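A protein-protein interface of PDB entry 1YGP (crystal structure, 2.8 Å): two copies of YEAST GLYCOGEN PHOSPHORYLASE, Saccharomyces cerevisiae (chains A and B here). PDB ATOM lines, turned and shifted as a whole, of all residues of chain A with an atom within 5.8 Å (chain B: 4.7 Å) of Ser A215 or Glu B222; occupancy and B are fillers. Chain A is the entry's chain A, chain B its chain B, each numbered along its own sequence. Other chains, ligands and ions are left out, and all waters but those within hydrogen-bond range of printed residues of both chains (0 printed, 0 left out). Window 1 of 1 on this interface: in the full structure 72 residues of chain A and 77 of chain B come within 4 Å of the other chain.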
ATOM      1  N   ARG A  58      19.474 -31.555   5.063  1.00  0.00           N
ATOM      2  CA  ARG A  58      18.652 -32.410   4.224  1.00  0.00           C
ATOM      3  C   ARG A  58      19.250 -33.816   4.147  1.00  0.00           C
ATOM      4  O   ARG A  58      20.306 -34.066   4.736  1.00  0.00           O
ATOM      5  CB  ARG A  58      18.639 -31.663   2.927  1.00  0.00           C
ATOM      6  CG  ARG A  58      17.758 -32.085   1.805  1.00  0.00           C
ATOM      7  CD  ARG A  58      16.408 -31.506   2.054  1.00  0.00           C
ATOM      8  NE  ARG A  58      16.445 -30.069   2.008  1.00  0.00           N
ATOM      9  CZ  ARG A  58      15.460 -29.401   1.417  1.00  0.00           C
ATOM     10  NH1 ARG A  58      14.417 -30.008   0.834  1.00  0.00           N
ATOM     11  NH2 ARG A  58      15.499 -28.072   1.476  1.00  0.00           N
ATOM     12  N   MET A  66      16.470 -29.025  -7.075  1.00  0.00           N
ATOM     13  CA  MET A  66      16.782 -27.706  -6.536  1.00  0.00           C
ATOM     14  C   MET A  66      17.813 -27.860  -5.413  1.00  0.00           C
ATOM     15  O   MET A  66      18.810 -27.134  -5.384  1.00  0.00           O
ATOM     16  CB  MET A  66      15.481 -27.080  -6.024  1.00  0.00           C
ATOM     17  CG  MET A  66      15.507 -25.683  -5.429  1.00  0.00           C
ATOM     18  SD  MET A  66      16.399 -24.530  -6.486  1.00  0.00           S
ATOM     19  CE  MET A  66      15.139 -24.144  -7.665  1.00  0.00           C
ATOM     20  N   GLU A  70      21.576 -26.141  -5.480  1.00  0.00           N
ATOM     21  CA  GLU A  70      22.048 -25.346  -4.356  1.00  0.00           C
ATOM     22  C   GLU A  70      23.360 -25.928  -3.793  1.00  0.00           C
ATOM     23  O   GLU A  70      24.360 -25.215  -3.662  1.00  0.00           O
ATOM     24  CB  GLU A  70      20.968 -25.352  -3.291  1.00  0.00           C
ATOM     25  CG  GLU A  70      20.378 -24.012  -2.940  1.00  0.00           C
ATOM     26  CD  GLU A  70      19.316 -23.491  -3.905  1.00  0.00           C
ATOM     27  OE1 GLU A  70      18.239 -24.091  -3.966  1.00  0.00           O
ATOM     28  OE2 GLU A  70      19.553 -22.467  -4.558  1.00  0.00           O
ATOM     29  N   TRP A 212      14.790 -13.232  -9.844  1.00  0.00           N
ATOM     30  CA  TRP A 212      15.915 -14.163  -9.852  1.00  0.00           C
ATOM     31  C   TRP A 212      16.575 -14.404  -8.485  1.00  0.00           C
ATOM     32  O   TRP A 212      17.358 -15.344  -8.357  1.00  0.00           O
ATOM     33  CB  TRP A 212      16.976 -13.676 -10.880  1.00  0.00           C
ATOM     34  CG  TRP A 212      17.744 -12.408 -10.535  1.00  0.00           C
ATOM     35  CD1 TRP A 212      17.138 -11.178 -10.521  1.00  0.00           C
ATOM     36  CD2 TRP A 212      19.053 -12.353 -10.156  1.00  0.00           C
ATOM     37  NE1 TRP A 212      18.058 -10.344 -10.109  1.00  0.00           N
ATOM     38  CE2 TRP A 212      19.204 -10.994  -9.882  1.00  0.00           C
ATOM     39  CE3 TRP A 212      20.136 -13.202  -9.992  1.00  0.00           C
ATOM     40  CZ2 TRP A 212      20.414 -10.469  -9.439  1.00  0.00           C
ATOM     41  CZ3 TRP A 212      21.356 -12.671  -9.551  1.00  0.00           C
ATOM     42  CH2 TRP A 212      21.500 -11.320  -9.271  1.00  0.00           C
ATOM     43  N   LEU A 213      16.345 -13.620  -7.414  1.00  0.00           N
ATOM     44  CA  LEU A 213      16.972 -13.899  -6.116  1.00  0.00           C
ATOM     45  C   LEU A 213      16.046 -14.568  -5.114  1.00  0.00           C
ATOM     46  O   LEU A 213      16.290 -14.576  -3.908  1.00  0.00           O
ATOM     47  CB  LEU A 213      17.506 -12.608  -5.515  1.00  0.00           C
ATOM     48  CG  LEU A 213      18.621 -11.998  -6.334  1.00  0.00           C
ATOM     49  CD1 LEU A 213      18.815 -10.540  -5.953  1.00  0.00           C
ATOM     50  CD2 LEU A 213      19.842 -12.883  -6.191  1.00  0.00           C
ATOM     51  N   ASN A 214      14.973 -15.210  -5.586  1.00  0.00           N
ATOM     52  CA  ASN A 214      13.989 -15.779  -4.680  1.00  0.00           C
ATOM     53  C   ASN A 214      14.504 -16.824  -3.733  1.00  0.00           C
ATOM     54  O   ASN A 214      13.961 -16.952  -2.639  1.00  0.00           O
ATOM     55  CB  ASN A 214      12.822 -16.443  -5.383  1.00  0.00           C
ATOM     56  CG  ASN A 214      11.544 -15.864  -4.797  1.00  0.00           C
ATOM     57  OD1 ASN A 214      10.637 -15.461  -5.528  1.00  0.00           O
ATOM     58  ND2 ASN A 214      11.387 -15.732  -3.482  1.00  0.00           N
ATOM     59  N   SER A 215      15.546 -17.552  -4.087  1.00  0.00           N
ATOM     60  CA  SER A 215      16.061 -18.564  -3.193  1.00  0.00           C
ATOM     61  C   SER A 215      17.527 -18.220  -3.084  1.00  0.00           C
ATOM     62  O   SER A 215      18.433 -18.997  -3.415  1.00  0.00           O
ATOM     63  CB  SER A 215      15.846 -19.928  -3.823  1.00  0.00           C
ATOM     64  OG  SER A 215      14.572 -20.025  -4.465  1.00  0.00           O
ATOM     65  N   GLY A 216      17.739 -16.968  -2.693  1.00  0.00           N
ATOM     66  CA  GLY A 216      19.082 -16.452  -2.511  1.00  0.00           C
ATOM     67  C   GLY A 216      19.852 -16.514  -3.812  1.00  0.00           C
ATOM     68  O   GLY A 216      19.242 -16.436  -4.873  1.00  0.00           O
ATOM     69  N   ASN A 217      21.164 -16.692  -3.727  1.00  0.00           N
ATOM     70  CA  ASN A 217      22.027 -16.734  -4.892  1.00  0.00           C
ATOM     71  C   ASN A 217      23.319 -17.420  -4.494  1.00  0.00           C
ATOM     72  O   ASN A 217      24.145 -16.798  -3.822  1.00  0.00           O
ATOM     73  CB  ASN A 217      22.356 -15.324  -5.373  1.00  0.00           C
ATOM     74  CG  ASN A 217      23.235 -15.315  -6.607  1.00  0.00           C
ATOM     75  OD1 ASN A 217      24.189 -16.070  -6.795  1.00  0.00           O
ATOM     76  ND2 ASN A 217      22.918 -14.428  -7.512  1.00  0.00           N
ATOM     77  N   PRO A 218      23.615 -18.655  -4.872  1.00  0.00           N
ATOM     78  CA  PRO A 218      24.731 -19.364  -4.307  1.00  0.00           C
ATOM     79  C   PRO A 218      26.037 -18.876  -4.888  1.00  0.00           C
ATOM     80  O   PRO A 218      27.067 -19.318  -4.404  1.00  0.00           O
ATOM     81  CB  PRO A 218      24.397 -20.809  -4.582  1.00  0.00           C
ATOM     82  CG  PRO A 218      23.751 -20.716  -5.933  1.00  0.00           C
ATOM     83  CD  PRO A 218      22.909 -19.452  -5.860  1.00  0.00           C
ATOM     84  N   GLU B 220      18.227 -21.173   8.700  1.00  0.00           N
ATOM     85  CA  GLU B 220      16.937 -21.568   8.202  1.00  0.00           C
ATOM     86  C   GLU B 220      17.092 -22.498   7.084  1.00  0.00           C
ATOM     87  O   GLU B 220      18.164 -22.632   6.485  1.00  0.00           O
ATOM     88  CB  GLU B 220      16.126 -20.414   7.671  1.00  0.00           C
ATOM     89  CG  GLU B 220      15.988 -19.274   8.565  1.00  0.00           C
ATOM     90  CD  GLU B 220      15.412 -18.033   7.910  1.00  0.00           C
ATOM     91  OE1 GLU B 220      15.951 -17.568   6.911  1.00  0.00           O
ATOM     92  OE2 GLU B 220      14.421 -17.532   8.430  1.00  0.00           O
ATOM     93  N   ILE B 221      15.981 -23.123   6.781  1.00  0.00           N
ATOM     94  CA  ILE B 221      15.900 -23.787   5.574  1.00  0.00           C
ATOM     95  C   ILE B 221      14.743 -22.980   4.986  1.00  0.00           C
ATOM     96  O   ILE B 221      13.634 -22.953   5.537  1.00  0.00           O
ATOM     97  CB  ILE B 221      15.500 -25.267   5.717  1.00  0.00           C
ATOM     98  CG1 ILE B 221      16.088 -26.021   6.862  1.00  0.00           C
ATOM     99  CG2 ILE B 221      15.975 -25.879   4.460  1.00  0.00           C
ATOM    100  CD1 ILE B 221      17.578 -26.319   6.829  1.00  0.00           C
ATOM    101  N   GLU B 222      14.944 -22.220   3.919  1.00  0.00           N
ATOM    102  CA  GLU B 222      13.863 -21.503   3.281  1.00  0.00           C
ATOM    103  C   GLU B 222      13.146 -22.536   2.502  1.00  0.00           C
ATOM    104  O   GLU B 222      13.785 -23.052   1.605  1.00  0.00           O
ATOM    105  CB  GLU B 222      14.428 -20.429   2.389  1.00  0.00           C
ATOM    106  CG  GLU B 222      13.353 -19.751   1.571  1.00  0.00           C
ATOM    107  CD  GLU B 222      13.807 -18.692   0.578  1.00  0.00           C
ATOM    108  OE1 GLU B 222      14.906 -18.788   0.031  1.00  0.00           O
ATOM    109  OE2 GLU B 222      13.038 -17.769   0.324  1.00  0.00           O
ATOM    110  N   ARG B 223      11.877 -22.901   2.768  1.00  0.00           N
ATOM    111  CA  ARG B 223      11.251 -23.924   2.007  1.00  0.00           C
ATOM    112  C   ARG B 223      10.409 -23.219   0.995  1.00  0.00           C
ATOM    113  O   ARG B 223       9.184 -23.164   1.068  1.00  0.00           O
ATOM    114  CB  ARG B 223      10.316 -24.870   2.796  1.00  0.00           C
ATOM    115  CG  ARG B 223      10.689 -25.293   4.153  1.00  0.00           C
ATOM    116  CD  ARG B 223      12.108 -25.776   4.310  1.00  0.00           C
ATOM    117  NE  ARG B 223      12.434 -26.903   3.510  1.00  0.00           N
ATOM    118  CZ  ARG B 223      12.833 -28.075   4.011  1.00  0.00           C
ATOM    119  NH1 ARG B 223      12.944 -28.296   5.276  1.00  0.00           N
ATOM    120  NH2 ARG B 223      13.195 -29.036   3.214  1.00  0.00           N
ATOM    121  N   ASN B 224      11.043 -22.707  -0.027  1.00  0.00           N
ATOM    122  CA  ASN B 224      10.341 -22.034  -1.076  1.00  0.00           C
ATOM    123  C   ASN B 224       9.253 -22.854  -1.694  1.00  0.00           C
ATOM    124  O   ASN B 224       8.427 -22.341  -2.410  1.00  0.00           O
ATOM    125  CB  ASN B 224      11.363 -21.616  -2.092  1.00  0.00           C
ATOM    126  CG  ASN B 224      11.260 -20.138  -2.405  1.00  0.00           C
ATOM    127  OD1 ASN B 224      11.177 -19.301  -1.558  1.00  0.00           O
ATOM    128  ND2 ASN B 224      11.274 -19.776  -3.641  1.00  0.00           N
ATOM    129  N   GLU B 225       9.316 -24.165  -1.432  1.00  0.00           N
ATOM    130  CA  GLU B 225       8.397 -25.177  -1.825  1.00  0.00           C
ATOM    131  C   GLU B 225       7.056 -25.089  -1.100  1.00  0.00           C
ATOM    132  O   GLU B 225       6.000 -25.253  -1.643  1.00  0.00           O
ATOM    133  CB  GLU B 225       8.990 -26.543  -1.555  1.00  0.00           C
ATOM    134  CG  GLU B 225      10.308 -26.893  -2.220  1.00  0.00           C
ATOM    135  CD  GLU B 225      11.538 -26.455  -1.521  1.00  0.00           C
ATOM    136  OE1 GLU B 225      12.006 -25.345  -1.755  1.00  0.00           O
ATOM    137  OE2 GLU B 225      12.045 -27.227  -0.741  1.00  0.00           O
ATOM    138  N   ALA B 261       7.006 -21.071   4.012  1.00  0.00           N
ATOM    139  CA  ALA B 261       7.609 -21.599   5.180  1.00  0.00           C
ATOM    140  C   ALA B 261       9.115 -21.487   5.187  1.00  0.00           C
ATOM    141  O   ALA B 261       9.792 -21.502   4.168  1.00  0.00           O
ATOM    142  CB  ALA B 261       7.301 -23.056   5.373  1.00  0.00           C
ATOM    143  N   TYR B 262       9.629 -21.346   6.354  1.00  0.00           N
ATOM    144  CA  TYR B 262      11.044 -21.346   6.629  1.00  0.00           C
ATOM    145  C   TYR B 262      11.189 -22.293   7.790  1.00  0.00           C
ATOM    146  O   TYR B 262      10.482 -22.185   8.777  1.00  0.00           O
ATOM    147  CB  TYR B 262      11.510 -19.974   6.986  1.00  0.00           C
ATOM    148  CG  TYR B 262      11.689 -19.007   5.850  1.00  0.00           C
ATOM    149  CD1 TYR B 262      10.566 -18.498   5.224  1.00  0.00           C
ATOM    150  CD2 TYR B 262      12.965 -18.621   5.426  1.00  0.00           C
ATOM    151  CE1 TYR B 262      10.706 -17.610   4.180  1.00  0.00           C
ATOM    152  CE2 TYR B 262      13.114 -17.723   4.373  1.00  0.00           C
ATOM    153  CZ  TYR B 262      11.975 -17.228   3.761  1.00  0.00           C
ATOM    154  OH  TYR B 262      12.075 -16.342   2.728  1.00  0.00           O
ATOM    155  N   ARG B 283       4.009 -13.270   1.451  1.00  0.00           N
ATOM    156  CA  ARG B 283       4.478 -12.800   0.184  1.00  0.00           C
ATOM    157  C   ARG B 283       3.265 -12.420  -0.610  1.00  0.00           C
ATOM    158  O   ARG B 283       2.177 -12.905  -0.291  1.00  0.00           O
ATOM    159  CB  ARG B 283       5.286 -13.875  -0.470  1.00  0.00           C
ATOM    160  CG  ARG B 283       6.662 -14.018   0.140  1.00  0.00           C
ATOM    161  CD  ARG B 283       7.523 -14.942  -0.676  1.00  0.00           C
ATOM    162  NE  ARG B 283       8.728 -15.414  -0.046  1.00  0.00           N
ATOM    163  CZ  ARG B 283       9.417 -16.488  -0.450  1.00  0.00           C
ATOM    164  NH1 ARG B 283       9.036 -17.181  -1.463  1.00  0.00           N
ATOM    165  NH2 ARG B 283      10.472 -16.930   0.199  1.00  0.00           N
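Hydrophobic or aromatic side chains of chain B within 4 Å of the printed part of chain A: Ile B221.
Of the 10 printed residues of chain A, 3 touch a printed residue of chain B.
Among the printed residues, Asp or Glu carboxylates within 4 Å of a Lys or Arg side-chain nitrogen of the other chain: Arg A58 with Glu B225 (3.98 Å).
Printed residues of chain B within 4 Å of Arg A58: Ile B221, Arg B223 and Glu B225.
Ser A215 touches just these residues of chain B: Glu B222 (3.4 Å) and Asn B224 (3.4 Å).
Of the printed residues of chain A, Ile B221 touches Arg A58.
Of chain A, only Asn A214 and Ser A215 come within 4 Å of Glu B222.
The nearest printed residue of chain B that does not touch Ser A215 is Glu B225 (6.5 Å).
The nearest residue of chain A that does not touch Glu B222 is Gly A216 (4.3 Å).
The nearest printed residue of chain A that does not touch Arg B223 is Ser A215 (7.6 Å).
The side-chain amide oxygen (OD1) of Asn B224 lies close to the side-chain carboxylate (OE2) of Glu B222 (3.1 Å).
OH of Tyr B262 sits at hydrogen-bond distance from OE2 of Glu B222 (3.0 Å).
OE2 of Glu B222 lies within salt-bridge range of NH2 of Arg B283, 2.7 Å away.
O of Ala B261 is in hydrogen-bond range of N of Arg B223.
OD1 of Asn B224 sits at hydrogen-bond distance from NH1 of Arg B283 (3.0 Å).
The side-chain hydroxyl (OH) of Tyr B262 sits at hydrogen-bond distance from the guanidinium group (NH2) of Arg B283 (3.1 Å).
The side-chain carboxylate (OE2) of Glu B225 is in salt-bridge range of the guanidinium group (NH1) of Arg A58 (3.98 Å).
The side-chain amide nitrogen of Asn A214 lies close to the guanidinium group of Arg B283, at 3.4 Å.
The side-chain hydroxyl (OG) of Ser A215 lies within hydrogen-bond range of the side-chain amide nitrogen (ND2) of Asn B224 (3.4 Å).
The guanidinium group (NH1) of Arg A58 sits close to the guanidinium group (NH2) of Arg B223 (2.8 Å).
The backbone carbonyl oxygen of Asn A214 lies close to the side-chain carboxylate of Glu B222 (3.2 Å).
Arg A58 touches Ile B221.
Asn A214 touches Asn B224.
Ser A215 touches Glu B222.
No position is printed for both chains.
Of the 8 pairs that touch across the chains among the printed residues, none has its exchanged pair printed and touching as well.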
